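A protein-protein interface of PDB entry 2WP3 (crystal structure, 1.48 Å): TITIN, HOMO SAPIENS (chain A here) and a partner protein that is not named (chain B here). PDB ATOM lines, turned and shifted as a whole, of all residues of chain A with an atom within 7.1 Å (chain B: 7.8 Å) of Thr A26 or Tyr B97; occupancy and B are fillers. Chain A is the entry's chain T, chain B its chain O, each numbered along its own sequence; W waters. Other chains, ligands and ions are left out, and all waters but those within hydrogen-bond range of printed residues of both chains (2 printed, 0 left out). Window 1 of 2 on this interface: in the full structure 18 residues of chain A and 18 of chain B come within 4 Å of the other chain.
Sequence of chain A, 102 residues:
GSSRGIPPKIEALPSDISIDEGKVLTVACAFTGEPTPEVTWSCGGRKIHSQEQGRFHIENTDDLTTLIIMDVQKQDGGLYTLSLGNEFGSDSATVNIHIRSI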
ATOM      1  N   LEU A  13     -12.966  -2.573  21.817  1.00  0.00           N
ATOM      2  CA  LEU A  13     -13.993  -2.077  22.741  1.00  0.00           C
ATOM      3  C   LEU A  13     -14.932  -1.231  21.941  1.00  0.00           C
ATOM      4  O   LEU A  13     -14.457  -0.475  21.116  1.00  0.00           O
ATOM      5  CB  LEU A  13     -13.313  -1.248  23.817  1.00  0.00           C
ATOM      6  CG  LEU A  13     -14.198  -0.758  24.975  1.00  0.00           C
ATOM      7  CD1 LEU A  13     -14.661  -1.922  25.905  1.00  0.00           C
ATOM      8  CD2 LEU A  13     -13.468   0.304  25.826  1.00  0.00           C
ATOM      9  N   PRO A  14     -16.295  -1.375  22.086  1.00  0.00           N
ATOM     10  CA  PRO A  14     -17.161  -0.531  21.319  1.00  0.00           C
ATOM     11  C   PRO A  14     -16.870   0.920  21.655  1.00  0.00           C
ATOM     12  O   PRO A  14     -16.562   1.241  22.823  1.00  0.00           O
ATOM     13  CB  PRO A  14     -18.580  -0.901  21.840  1.00  0.00           C
ATOM     14  CG  PRO A  14     -18.439  -2.264  22.402  1.00  0.00           C
ATOM     15  CD  PRO A  14     -17.060  -2.310  22.950  1.00  0.00           C
ATOM     16  N   ASP A  16     -19.270   3.309  21.423  1.00  0.00           N
ATOM     17  CA  ASP A  16     -20.535   3.821  21.935  1.00  0.00           C
ATOM     18  C   ASP A  16     -21.483   2.665  22.188  1.00  0.00           C
ATOM     19  O   ASP A  16     -21.572   1.691  21.380  1.00  0.00           O
ATOM     20  CB  ASP A  16     -21.218   4.757  20.949  1.00  0.00           C
ATOM     21  CG  ASP A  16     -20.456   6.034  20.752  1.00  0.00           C
ATOM     22  OD1 ASP A  16     -19.549   6.069  19.877  1.00  0.00           O
ATOM     23  OD2 ASP A  16     -20.798   7.001  21.451  1.00  0.00           O
ATOM     24  N   ILE A  17     -22.171   2.743  23.323  1.00  0.00           N
ATOM     25  CA  ILE A  17     -23.146   1.707  23.682  1.00  0.00           C
ATOM     26  C   ILE A  17     -24.335   2.375  24.319  1.00  0.00           C
ATOM     27  O   ILE A  17     -24.217   3.492  24.815  1.00  0.00           O
ATOM     28  CB  ILE A  17     -22.534   0.553  24.583  1.00  0.00           C
ATOM     29  CG1 ILE A  17     -22.177   0.980  26.001  1.00  0.00           C
ATOM     30  CG2 ILE A  17     -21.315  -0.102  23.944  1.00  0.00           C
ATOM     31  CD1 ILE A  17     -21.415  -0.135  26.764  1.00  0.00           C
ATOM     32  N   SER A  18     -25.474   1.669  24.306  1.00  0.00           N
ATOM     33  CA  SER A  18     -26.726   2.225  24.840  1.00  0.00           C
ATOM     34  C   SER A  18     -27.496   1.186  25.696  1.00  0.00           C
ATOM     35  O   SER A  18     -27.318  -0.046  25.592  1.00  0.00           O
ATOM     36  CB  SER A  18     -27.563   2.827  23.730  1.00  0.00           C
ATOM     37  OG  SER A  18     -27.072   4.109  23.267  1.00  0.00           O
ATOM     38  N   ILE A  19     -28.266   1.715  26.636  1.00  0.00           N
ATOM     39  CA  ILE A  19     -29.039   0.925  27.525  1.00  0.00           C
ATOM     40  C   ILE A  19     -30.239   1.796  27.935  1.00  0.00           C
ATOM     41  O   ILE A  19     -30.182   3.046  27.967  1.00  0.00           O
ATOM     42  CB  ILE A  19     -28.167   0.447  28.733  1.00  0.00           C
ATOM     43  CG1 ILE A  19     -28.935  -0.547  29.630  1.00  0.00           C
ATOM     44  CG2 ILE A  19     -27.793   1.619  29.601  1.00  0.00           C
ATOM     45  CD1 ILE A  19     -29.351  -1.852  29.037  1.00  0.00           C
ATOM     46  N   VAL A  24     -30.196  -3.908  32.748  1.00  0.00           N
ATOM     47  CA  VAL A  24     -28.840  -4.330  33.081  1.00  0.00           C
ATOM     48  C   VAL A  24     -27.950  -4.167  31.842  1.00  0.00           C
ATOM     49  O   VAL A  24     -28.315  -4.680  30.758  1.00  0.00           O
ATOM     50  CB  VAL A  24     -28.835  -5.800  33.570  1.00  0.00           C
ATOM     51  CG1 VAL A  24     -27.404  -6.305  33.775  1.00  0.00           C
ATOM     52  CG2 VAL A  24     -29.663  -5.947  34.853  1.00  0.00           C
ATOM     53  N   LEU A  25     -26.816  -3.496  31.997  1.00  0.00           N
ATOM     54  CA  LEU A  25     -25.855  -3.368  30.908  1.00  0.00           C
ATOM     55  C   LEU A  25     -24.631  -4.205  31.239  1.00  0.00           C
ATOM     56  O   LEU A  25     -24.064  -4.091  32.343  1.00  0.00           O
ATOM     57  CB  LEU A  25     -25.479  -1.902  30.691  1.00  0.00           C
ATOM     58  CG  LEU A  25     -24.395  -1.635  29.660  1.00  0.00           C
ATOM     59  CD1 LEU A  25     -24.872  -2.083  28.255  1.00  0.00           C
ATOM     60  CD2 LEU A  25     -24.095  -0.125  29.660  1.00  0.00           C
ATOM     61  N   THR A  26     -24.171  -5.004  30.274  1.00  0.00           N
ATOM     62  CA  THR A  26     -22.922  -5.770  30.381  1.00  0.00           C
ATOM     63  C   THR A  26     -22.014  -5.384  29.187  1.00  0.00           C
ATOM     64  O   THR A  26     -22.461  -5.414  28.060  1.00  0.00           O
ATOM     65  CB  THR A  26     -23.219  -7.258  30.338  1.00  0.00           C
ATOM     66  OG1 THR A  26     -24.027  -7.581  31.469  1.00  0.00           O
ATOM     67  CG2 THR A  26     -21.922  -8.097  30.401  1.00  0.00           C
ATOM     68  N   VAL A  27     -20.788  -4.941  29.465  1.00  0.00           N
ATOM     69  CA  VAL A  27     -19.761  -4.754  28.399  1.00  0.00           C
ATOM     70  C   VAL A  27     -18.538  -5.559  28.768  1.00  0.00           C
ATOM     71  O   VAL A  27     -17.989  -5.415  29.865  1.00  0.00           O
ATOM     72  CB  VAL A  27     -19.455  -3.259  28.084  1.00  0.00           C
ATOM     73  CG1 VAL A  27     -19.092  -2.516  29.285  1.00  0.00           C
ATOM     74  CG2 VAL A  27     -18.351  -3.098  26.991  1.00  0.00           C
ATOM     75  N   ALA A  28     -18.104  -6.406  27.845  1.00  0.00           N
ATOM     76  CA  ALA A  28     -16.986  -7.319  28.092  1.00  0.00           C
ATOM     77  C   ALA A  28     -15.874  -6.948  27.126  1.00  0.00           C
ATOM     78  O   ALA A  28     -16.153  -6.574  25.971  1.00  0.00           O
ATOM     79  CB  ALA A  28     -17.401  -8.791  27.893  1.00  0.00           C
ATOM     80  N   CYS A  29     -14.618  -7.120  27.535  1.00  0.00           N
ATOM     81  CA  CYS A  29     -13.476  -6.730  26.699  1.00  0.00           C
ATOM     82  C   CYS A  29     -12.299  -7.647  27.019  1.00  0.00           C
ATOM     83  O   CYS A  29     -11.947  -7.842  28.193  1.00  0.00           O
ATOM     84  CB  CYS A  29     -13.129  -5.271  26.950  1.00  0.00           C
ATOM     85  SG  CYS A  29     -11.863  -4.578  25.864  1.00  0.00           S
ATOM     86  N   THR A  66     -15.138  -7.600  32.495  1.00  0.00           N
ATOM     87  CA  THR A  66     -16.553  -7.404  32.245  1.00  0.00           C
ATOM     88  C   THR A  66     -17.087  -6.389  33.251  1.00  0.00           C
ATOM     89  O   THR A  66     -16.959  -6.560  34.459  1.00  0.00           O
ATOM     90  CB  THR A  66     -17.320  -8.744  32.336  1.00  0.00           C
ATOM     91  OG1 THR A  66     -16.781  -9.708  31.427  1.00  0.00           O
ATOM     92  CG2 THR A  66     -18.792  -8.519  31.999  1.00  0.00           C
ATOM     93  N   LEU A  67     -17.683  -5.322  32.729  1.00  0.00           N
ATOM     94  CA  LEU A  67     -18.375  -4.319  33.529  1.00  0.00           C
ATOM     95  C   LEU A  67     -19.860  -4.578  33.438  1.00  0.00           C
ATOM     96  O   LEU A  67     -20.425  -4.706  32.326  1.00  0.00           O
ATOM     97  CB  LEU A  67     -18.046  -2.956  33.025  1.00  0.00           C
ATOM     98  CG  LEU A  67     -18.810  -1.745  33.574  1.00  0.00           C
ATOM     99  CD1 LEU A  67     -18.411  -1.493  35.014  1.00  0.00           C
ATOM    100  CD2 LEU A  67     -18.599  -0.498  32.742  1.00  0.00           C
ATOM    101  N   ILE A  68     -20.519  -4.656  34.616  1.00  0.00           N
ATOM    102  CA  ILE A  68     -21.947  -4.928  34.706  1.00  0.00           C
ATOM    103  C   ILE A  68     -22.564  -3.790  35.507  1.00  0.00           C
ATOM    104  O   ILE A  68     -22.084  -3.483  36.611  1.00  0.00           O
ATOM    105  CB  ILE A  68     -22.277  -6.320  35.362  1.00  0.00           C
ATOM    106  CG1 ILE A  68     -21.500  -7.431  34.661  1.00  0.00           C
ATOM    107  CG2 ILE A  68     -23.809  -6.578  35.279  1.00  0.00           C
ATOM    108  CD1 ILE A  68     -21.523  -8.759  35.394  1.00  0.00           C
ATOM    109  N   ILE A  69     -23.539  -3.092  34.909  1.00  0.00           N
ATOM    110  CA  ILE A  69     -24.271  -2.063  35.619  1.00  0.00           C
ATOM    111  C   ILE A  69     -25.728  -2.528  35.772  1.00  0.00           C
ATOM    112  O   ILE A  69     -26.461  -2.680  34.777  1.00  0.00           O
ATOM    113  CB  ILE A  69     -24.274  -0.692  34.936  1.00  0.00           C
ATOM    114  CG1 ILE A  69     -22.830  -0.325  34.467  1.00  0.00           C
ATOM    115  CG2 ILE A  69     -24.835   0.364  35.922  1.00  0.00           C
ATOM    116  CD1 ILE A  69     -22.762   0.991  33.744  1.00  0.00           C
ATOM    117  N   MET A  70     -26.132  -2.809  37.005  1.00  0.00           N
ATOM    118  CA  MET A  70     -27.500  -3.201  37.306  1.00  0.00           C
ATOM    119  C   MET A  70     -28.394  -1.975  37.443  1.00  0.00           C
ATOM    120  O   MET A  70     -27.943  -0.937  37.870  1.00  0.00           O
ATOM    121  CB  MET A  70     -27.573  -3.986  38.621  1.00  0.00           C
ATOM    122  CG  MET A  70     -26.656  -5.207  38.727  1.00  0.00           C
ATOM    123  SD  MET A  70     -27.005  -6.570  37.585  1.00  0.00           S
ATOM    124  CE  MET A  70     -25.820  -7.800  38.146  1.00  0.00           C
ATOM    125  N   VAL A  95     -15.315   3.924  26.086  1.00  0.00           N
ATOM    126  CA  VAL A  95     -16.652   3.631  25.598  1.00  0.00           C
ATOM    127  C   VAL A  95     -17.585   4.651  26.187  1.00  0.00           C
ATOM    128  O   VAL A  95     -17.632   4.906  27.381  1.00  0.00           O
ATOM    129  CB  VAL A  95     -17.061   2.150  25.934  1.00  0.00           C
ATOM    130  CG1 VAL A  95     -16.979   1.814  27.449  1.00  0.00           C
ATOM    131  CG2 VAL A  95     -18.406   1.856  25.360  1.00  0.00           C
ATOM    132  N   ARG A 100     -30.780   5.880  27.554  1.00  0.00           N
ATOM    133  CA  ARG A 100     -32.026   6.313  26.904  1.00  0.00           C
ATOM    134  C   ARG A 100     -33.167   6.409  27.938  1.00  0.00           C
ATOM    135  O   ARG A 100     -33.476   5.432  28.673  1.00  0.00           O
ATOM    136  CB  ARG A 100     -32.469   5.335  25.802  1.00  0.00           C
ATOM    137  CG  ARG A 100     -31.417   4.867  24.795  1.00  0.00           C
ATOM    138  CD  ARG A 100     -32.093   3.999  23.703  1.00  0.00           C
ATOM    139  NE  ARG A 100     -31.265   2.890  23.196  1.00  0.00           N
ATOM    140  CZ  ARG A 100     -31.119   1.691  23.777  1.00  0.00           C
ATOM    141  NH1 ARG A 100     -31.750   1.399  24.910  1.00  0.00           N
ATOM    142  NH2 ARG A 100     -30.324   0.768  23.230  1.00  0.00           N
ATOM    143  N   PRO B  14     -30.832 -11.061  32.080  1.00  0.00           N
ATOM    144  CA  PRO B  14     -30.179 -10.333  30.986  1.00  0.00           C
ATOM    145  C   PRO B  14     -29.085 -11.061  30.221  1.00  0.00           C
ATOM    146  O   PRO B  14     -28.545 -12.099  30.674  1.00  0.00           O
ATOM    147  CB  PRO B  14     -29.662  -9.047  31.657  1.00  0.00           C
ATOM    148  CG  PRO B  14     -29.405  -9.449  33.056  1.00  0.00           C
ATOM    149  CD  PRO B  14     -30.531 -10.458  33.400  1.00  0.00           C
ATOM    150  N   PRO B  15     -28.748 -10.546  29.036  1.00  0.00           N
ATOM    151  CA  PRO B  15     -27.853 -11.257  28.161  1.00  0.00           C
ATOM    152  C   PRO B  15     -26.448 -11.263  28.749  1.00  0.00           C
ATOM    153  O   PRO B  15     -26.070 -10.304  29.422  1.00  0.00           O
ATOM    154  CB  PRO B  15     -27.917 -10.475  26.880  1.00  0.00           C
ATOM    155  CG  PRO B  15     -29.140  -9.672  26.943  1.00  0.00           C
ATOM    156  CD  PRO B  15     -29.364  -9.405  28.377  1.00  0.00           C
ATOM    157  N   CYS B  16     -25.732 -12.316  28.501  1.00  0.00           N
ATOM    158  CA  CYS B  16     -24.317 -12.409  28.874  1.00  0.00           C
ATOM    159  C   CYS B  16     -23.623 -13.323  27.903  1.00  0.00           C
ATOM    160  O   CYS B  16     -24.268 -14.029  27.097  1.00  0.00           O
ATOM    161  CB  CYS B  16     -24.207 -12.958  30.267  1.00  0.00           C
ATOM    162  SG  CYS B  16     -25.046 -14.493  30.421  1.00  0.00           S
ATOM    163  N   PHE B  17     -22.301 -13.257  27.919  1.00  0.00           N
ATOM    164  CA  PHE B  17     -21.478 -14.121  27.101  1.00  0.00           C
ATOM    165  C   PHE B  17     -20.946 -15.336  27.779  1.00  0.00           C
ATOM    166  O   PHE B  17     -20.217 -15.264  28.821  1.00  0.00           O
ATOM    167  CB  PHE B  17     -20.296 -13.293  26.568  1.00  0.00           C
ATOM    168  CG  PHE B  17     -20.727 -12.107  25.854  1.00  0.00           C
ATOM    169  CD1 PHE B  17     -21.295 -12.231  24.623  1.00  0.00           C
ATOM    170  CD2 PHE B  17     -20.697 -10.839  26.465  1.00  0.00           C
ATOM    171  CE1 PHE B  17     -21.787 -11.078  23.966  1.00  0.00           C
ATOM    172  CE2 PHE B  17     -21.124  -9.719  25.800  1.00  0.00           C
ATOM    173  CZ  PHE B  17     -21.678  -9.849  24.547  1.00  0.00           C
ATOM    174  N   PHE B  20     -16.764 -15.555  24.471  1.00  0.00           N
ATOM    175  CA  PHE B  20     -16.501 -14.201  24.016  1.00  0.00           C
ATOM    176  C   PHE B  20     -15.831 -14.266  22.647  1.00  0.00           C
ATOM    177  O   PHE B  20     -15.043 -15.169  22.374  1.00  0.00           O
ATOM    178  CB  PHE B  20     -15.606 -13.473  25.045  1.00  0.00           C
ATOM    179  CG  PHE B  20     -15.329 -12.006  24.698  1.00  0.00           C
ATOM    180  CD1 PHE B  20     -16.145 -11.016  25.183  1.00  0.00           C
ATOM    181  CD2 PHE B  20     -14.253 -11.649  23.899  1.00  0.00           C
ATOM    182  CE1 PHE B  20     -15.929  -9.651  24.855  1.00  0.00           C
ATOM    183  CE2 PHE B  20     -14.013 -10.309  23.563  1.00  0.00           C
ATOM    184  CZ  PHE B  20     -14.844  -9.301  24.053  1.00  0.00           C
ATOM    185  N   PRO B  21     -16.174 -13.309  21.753  1.00  0.00           N
ATOM    186  CA  PRO B  21     -15.634 -13.344  20.402  1.00  0.00           C
ATOM    187  C   PRO B  21     -14.213 -12.897  20.377  1.00  0.00           C
ATOM    188  O   PRO B  21     -13.931 -11.707  20.646  1.00  0.00           O
ATOM    189  CB  PRO B  21     -16.491 -12.323  19.645  1.00  0.00           C
ATOM    190  CG  PRO B  21     -17.004 -11.421  20.643  1.00  0.00           C
ATOM    191  CD  PRO B  21     -17.172 -12.238  21.903  1.00  0.00           C
ATOM    192  N   VAL B  47     -27.111  -9.077  17.296  1.00  0.00           N
ATOM    193  CA  VAL B  47     -26.819  -8.397  16.075  1.00  0.00           C
ATOM    194  C   VAL B  47     -25.333  -8.275  16.023  1.00  0.00           C
ATOM    195  O   VAL B  47     -24.623  -8.273  17.044  1.00  0.00           O
ATOM    196  CB  VAL B  47     -27.353  -6.951  16.028  1.00  0.00           C
ATOM    197  CG1 VAL B  47     -28.770  -6.825  16.586  1.00  0.00           C
ATOM    198  CG2 VAL B  47     -26.372  -6.022  16.726  1.00  0.00           C
ATOM    199  N   GLU B  49     -22.781  -5.427  14.315  1.00  0.00           N
ATOM    200  CA  GLU B  49     -22.661  -4.075  13.810  1.00  0.00           C
ATOM    201  C   GLU B  49     -21.211  -3.789  13.437  1.00  0.00           C
ATOM    202  O   GLU B  49     -20.321  -4.421  13.934  1.00  0.00           O
ATOM    203  CB  GLU B  49     -23.191  -3.063  14.865  1.00  0.00           C
ATOM    204  CG  GLU B  49     -24.643  -3.344  15.254  1.00  0.00           C
ATOM    205  CD  GLU B  49     -25.234  -2.357  16.247  1.00  0.00           C
ATOM    206  OE1 GLU B  49     -24.457  -1.576  16.829  1.00  0.00           O
ATOM    207  OE2 GLU B  49     -26.482  -2.357  16.448  1.00  0.00           O
ATOM    208  N   VAL B  86     -18.931  -5.299  16.426  1.00  0.00           N
ATOM    209  CA  VAL B  86     -19.574  -5.328  17.725  1.00  0.00           C
ATOM    210  C   VAL B  86     -20.755  -6.302  17.710  1.00  0.00           C
ATOM    211  O   VAL B  86     -21.643  -6.199  16.811  1.00  0.00           O
ATOM    212  CB  VAL B  86     -20.089  -3.941  18.135  1.00  0.00           C
ATOM    213  CG1 VAL B  86     -20.808  -4.090  19.515  1.00  0.00           C
ATOM    214  CG2 VAL B  86     -18.951  -2.867  18.290  1.00  0.00           C
ATOM    215  N   CYS B  87     -20.708  -7.244  18.672  1.00  0.00           N
ATOM    216  CA  CYS B  87     -21.814  -8.178  18.909  1.00  0.00           C
ATOM    217  C   CYS B  87     -22.673  -7.604  20.021  1.00  0.00           C
ATOM    218  O   CYS B  87     -22.199  -7.452  21.133  1.00  0.00           O
ATOM    219  CB  CYS B  87     -21.322  -9.557  19.314  1.00  0.00           C
ATOM    220  SG  CYS B  87     -22.690 -10.744  19.379  1.00  0.00           S
ATOM    221  N   ARG B  88     -23.900  -7.248  19.688  1.00  0.00           N
ATOM    222  CA  ARG B  88     -24.843  -6.613  20.588  1.00  0.00           C
ATOM    223  C   ARG B  88     -25.991  -7.586  20.834  1.00  0.00           C
ATOM    224  O   ARG B  88     -26.650  -7.997  19.891  1.00  0.00           O
ATOM    225  CB  ARG B  88     -25.295  -5.325  19.965  1.00  0.00           C
ATOM    226  CG  ARG B  88     -26.304  -4.582  20.755  1.00  0.00           C
ATOM    227  CD  ARG B  88     -26.804  -3.378  19.976  1.00  0.00           C
ATOM    228  NE  ARG B  88     -27.861  -2.678  20.687  1.00  0.00           N
ATOM    229  CZ  ARG B  88     -28.512  -1.652  20.161  1.00  0.00           C
ATOM    230  NH1 ARG B  88     -28.194  -1.248  18.928  1.00  0.00           N
ATOM    231  NH2 ARG B  88     -29.461  -1.038  20.853  1.00  0.00           N
ATOM    232  N   ALA B  89     -26.167  -8.021  22.085  1.00  0.00           N
ATOM    233  CA  ALA B  89     -27.260  -8.950  22.498  1.00  0.00           C
ATOM    234  C   ALA B  89     -28.290  -8.174  23.307  1.00  0.00           C
ATOM    235  O   ALA B  89     -27.891  -7.388  24.159  1.00  0.00           O
ATOM    236  CB  ALA B  89     -26.686 -10.030  23.334  1.00  0.00           C
ATOM    237  N   ARG B  90     -29.584  -8.336  23.016  1.00  0.00           N
ATOM    238  CA  ARG B  90     -30.634  -7.681  23.775  1.00  0.00           C
ATOM    239  C   ARG B  90     -31.753  -8.674  24.136  1.00  0.00           C
ATOM    240  O   ARG B  90     -32.044  -9.604  23.366  1.00  0.00           O
ATOM    241  CB  ARG B  90     -31.250  -6.523  22.977  1.00  0.00           C
ATOM    242  CG  ARG B  90     -30.277  -5.448  22.459  1.00  0.00           C
ATOM    243  CD  ARG B  90     -30.990  -4.501  21.502  1.00  0.00           C
ATOM    244  NE  ARG B  90     -30.704  -4.918  20.142  1.00  0.00           N
ATOM    245  CZ  ARG B  90     -31.062  -4.264  19.056  1.00  0.00           C
ATOM    246  NH1 ARG B  90     -30.714  -4.750  17.881  1.00  0.00           N
ATOM    247  NH2 ARG B  90     -31.756  -3.141  19.151  1.00  0.00           N
ATOM    248  N   GLY B  94     -32.114  -6.687  29.584  1.00  0.00           N
ATOM    249  CA  GLY B  94     -30.885  -5.848  29.384  1.00  0.00           C
ATOM    250  C   GLY B  94     -30.168  -6.060  28.073  1.00  0.00           C
ATOM    251  O   GLY B  94     -30.715  -6.642  27.130  1.00  0.00           O
ATOM    252  N   GLU B  95     -28.917  -5.599  28.034  1.00  0.00           N
ATOM    253  CA  GLU B  95     -28.106  -5.649  26.826  1.00  0.00           C
ATOM    254  C   GLU B  95     -26.693  -6.057  27.201  1.00  0.00           C
ATOM    255  O   GLU B  95     -26.253  -5.743  28.354  1.00  0.00           O
ATOM    256  CB  GLU B  95     -28.107  -4.301  26.103  1.00  0.00           C
ATOM    257  CG  GLU B  95     -29.511  -3.804  25.798  1.00  0.00           C
ATOM    258  CD  GLU B  95     -29.578  -2.607  24.876  1.00  0.00           C
ATOM    259  OE1 GLU B  95     -30.412  -1.722  25.127  1.00  0.00           O
ATOM    260  OE2 GLU B  95     -28.769  -2.514  23.959  1.00  0.00           O
ATOM    261  N   ALA B  96     -25.998  -6.764  26.307  1.00  0.00           N
ATOM    262  CA  ALA B  96     -24.600  -7.078  26.471  1.00  0.00           C
ATOM    263  C   ALA B  96     -23.824  -6.796  25.164  1.00  0.00           C
ATOM    264  O   ALA B  96     -24.368  -7.018  24.084  1.00  0.00           O
ATOM    265  CB  ALA B  96     -24.407  -8.519  26.874  1.00  0.00           C
ATOM    266  N   TYR B  97     -22.599  -6.300  25.300  1.00  0.00           N
ATOM    267  CA  TYR B  97     -21.799  -5.824  24.158  1.00  0.00           C
ATOM    268  C   TYR B  97     -20.424  -6.430  24.219  1.00  0.00           C
ATOM    269  O   TYR B  97     -19.809  -6.481  25.264  1.00  0.00           O
ATOM    270  CB  TYR B  97     -21.707  -4.276  24.141  1.00  0.00           C
ATOM    271  CG  TYR B  97     -22.963  -3.485  23.877  1.00  0.00           C
ATOM    272  CD1 TYR B  97     -23.197  -2.952  22.609  1.00  0.00           C
ATOM    273  CD2 TYR B  97     -23.918  -3.279  24.856  1.00  0.00           C
ATOM    274  CE1 TYR B  97     -24.326  -2.179  22.369  1.00  0.00           C
ATOM    275  CE2 TYR B  97     -25.034  -2.516  24.615  1.00  0.00           C
ATOM    276  CZ  TYR B  97     -25.247  -2.004  23.342  1.00  0.00           C
ATOM    277  OH  TYR B  97     -26.384  -1.251  23.138  1.00  0.00           O
ATOM    278  N   ALA B  98     -19.921  -6.898  23.064  1.00  0.00           N
ATOM    279  CA  ALA B  98     -18.570  -7.399  22.978  1.00  0.00           C
ATOM    280  C   ALA B  98     -18.085  -6.990  21.615  1.00  0.00           C
ATOM    281  O   ALA B  98     -18.759  -7.234  20.622  1.00  0.00           O
ATOM    282  CB  ALA B  98     -18.536  -8.907  23.116  1.00  0.00           C
ATOM    283  N   ALA B  99     -16.901  -6.371  21.575  1.00  0.00           N
ATOM    284  CA  ALA B  99     -16.240  -6.078  20.295  1.00  0.00           C
ATOM    285  C   ALA B  99     -15.092  -7.033  19.964  1.00  0.00           C
ATOM    286  O   ALA B  99     -14.447  -7.575  20.831  1.00  0.00           O
ATOM    287  CB  ALA B  99     -15.759  -4.634  20.245  1.00  0.00           C
HETATM  288  O   HOH W   1     -26.580  -7.709  30.467  1.00  0.00           O
HETATM  289  O   HOH W   2     -15.422  -5.211  23.716  1.00  0.00           O
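N of Glu B95 sits at hydrogen-bond distance from O of Val A24.
N of Thr A26 sits at hydrogen-bond distance from O of Glu B95, 2.9 Å away.
OE1 of Glu B95 is in salt-bridge range of NH2 of Arg A100 (3.1 Å).
The side-chain hydroxyl (OH) of Tyr B97 is in hydrogen-bond range of the backbone carbonyl oxygen (O) of Ser A18 (2.9 Å).
The backbone carbonyl oxygen (O) of Thr A26 lies within hydrogen-bond range of the backbone NH (N) of Tyr B97 (2.9 Å).
O of Tyr B97 lies within hydrogen-bond range of N of Ala A28, at 3.1 Å.
The backbone carbonyl oxygen (O) of Ser A18 sits close to the side-chain carboxylate (OE2) of Glu B95, at 3.3 Å.
The guanidinium group (NH2) of Arg A100 lies close to the guanidinium group (NH2) of Arg B88, 3.1 Å away.
The guanidinium group of Arg B88 is in salt-bridge range of the side-chain carboxylate of Glu B49.
The guanidinium group of Arg B88 is in salt-bridge range of the side-chain carboxylate of Glu B95 (3.4 Å).
The backbone NH (N) of Ala B89 sits at hydrogen-bond distance from the backbone carbonyl oxygen (O) of Ala B96, at 2.9 Å.
OE2 of Glu B95 sits at hydrogen-bond distance from OH of Tyr B97.
O of Ile A19 is in hydrogen-bond range of N of Arg A100.
The backbone carbonyl oxygen of Leu A25 lies within hydrogen-bond range of the backbone NH of Ile A69, at 2.8 Å.
N of Leu A13 touches CB of Ala B99 (3.8 Å).
Ala B99 touches Pro A14.
Ile A17 touches Tyr B97 (CG2 to CD1, 3.7 Å).
Glu B95 touches Ile A19.
CA of Leu A25 touches O of Glu B95 (3.5 Å).
Leu A25 touches Tyr B97.
Val A27 touches Tyr B97 (CA to O, 3.6 Å).
O of Ala A28 touches CE1 of Phe B20, 3.3 Å away.
Ala A28 touches Ala B98.
Cys A29 touches Phe B20 (N to CE1, 3.9 Å).
Printed residues of chain B within 4 Å of Leu A13: Ala B99 (3.8 Å).
Of the printed residues of chain B, Ile A17 touches Tyr B97 (3.7 Å).
Thr A26 touches just these residues of chain B: Pro B15, Glu B95, Ala B96 and Tyr B97.
Of the printed residues of chain B, Val A27 touches Tyr B97 (3.6 Å).
Thr A66 touches none of the printed residues of chain B.
Ile A69 touches none of the printed residues of chain B.
Of the printed residues of chain A, Tyr B97 touches Ile A17, Ser A18, Leu A25, Thr A26, Val A27 and Ala A28.
Printed residues of chain A within 4 Å of Ala B98: Ala A28.
The nearest residue of chain B that does not touch Thr A26 is Phe B17 (4.9 Å).
The nearest printed residue of chain A that does not touch Phe B20 is Val A27 (6.2 Å).
Hydrophobic or aromatic side chains of chain A that line the printed part of chain B: Pro A14, Ile A17, Ile A19, Val A24, Leu A25 and Ala A28.
Hydrophobic or aromatic side chains of chain B within 4 Å of the printed part of chain A: Pro B14, Phe B20, Ala B96, Tyr B97 and Ala B99.
Water W2 bridges O of Ala A28 (2.7 Å) and N of Ala B99 (2.8 Å).
Water W1 lies within hydrogen-bond range of the side-chain hydroxyl (OG1) of Thr A26 (2.7 Å), the backbone carbonyl oxygen (O) of Pro B15 (2.8 Å) and the backbone carbonyl oxygen (O) of Glu B95 (2.9 Å).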
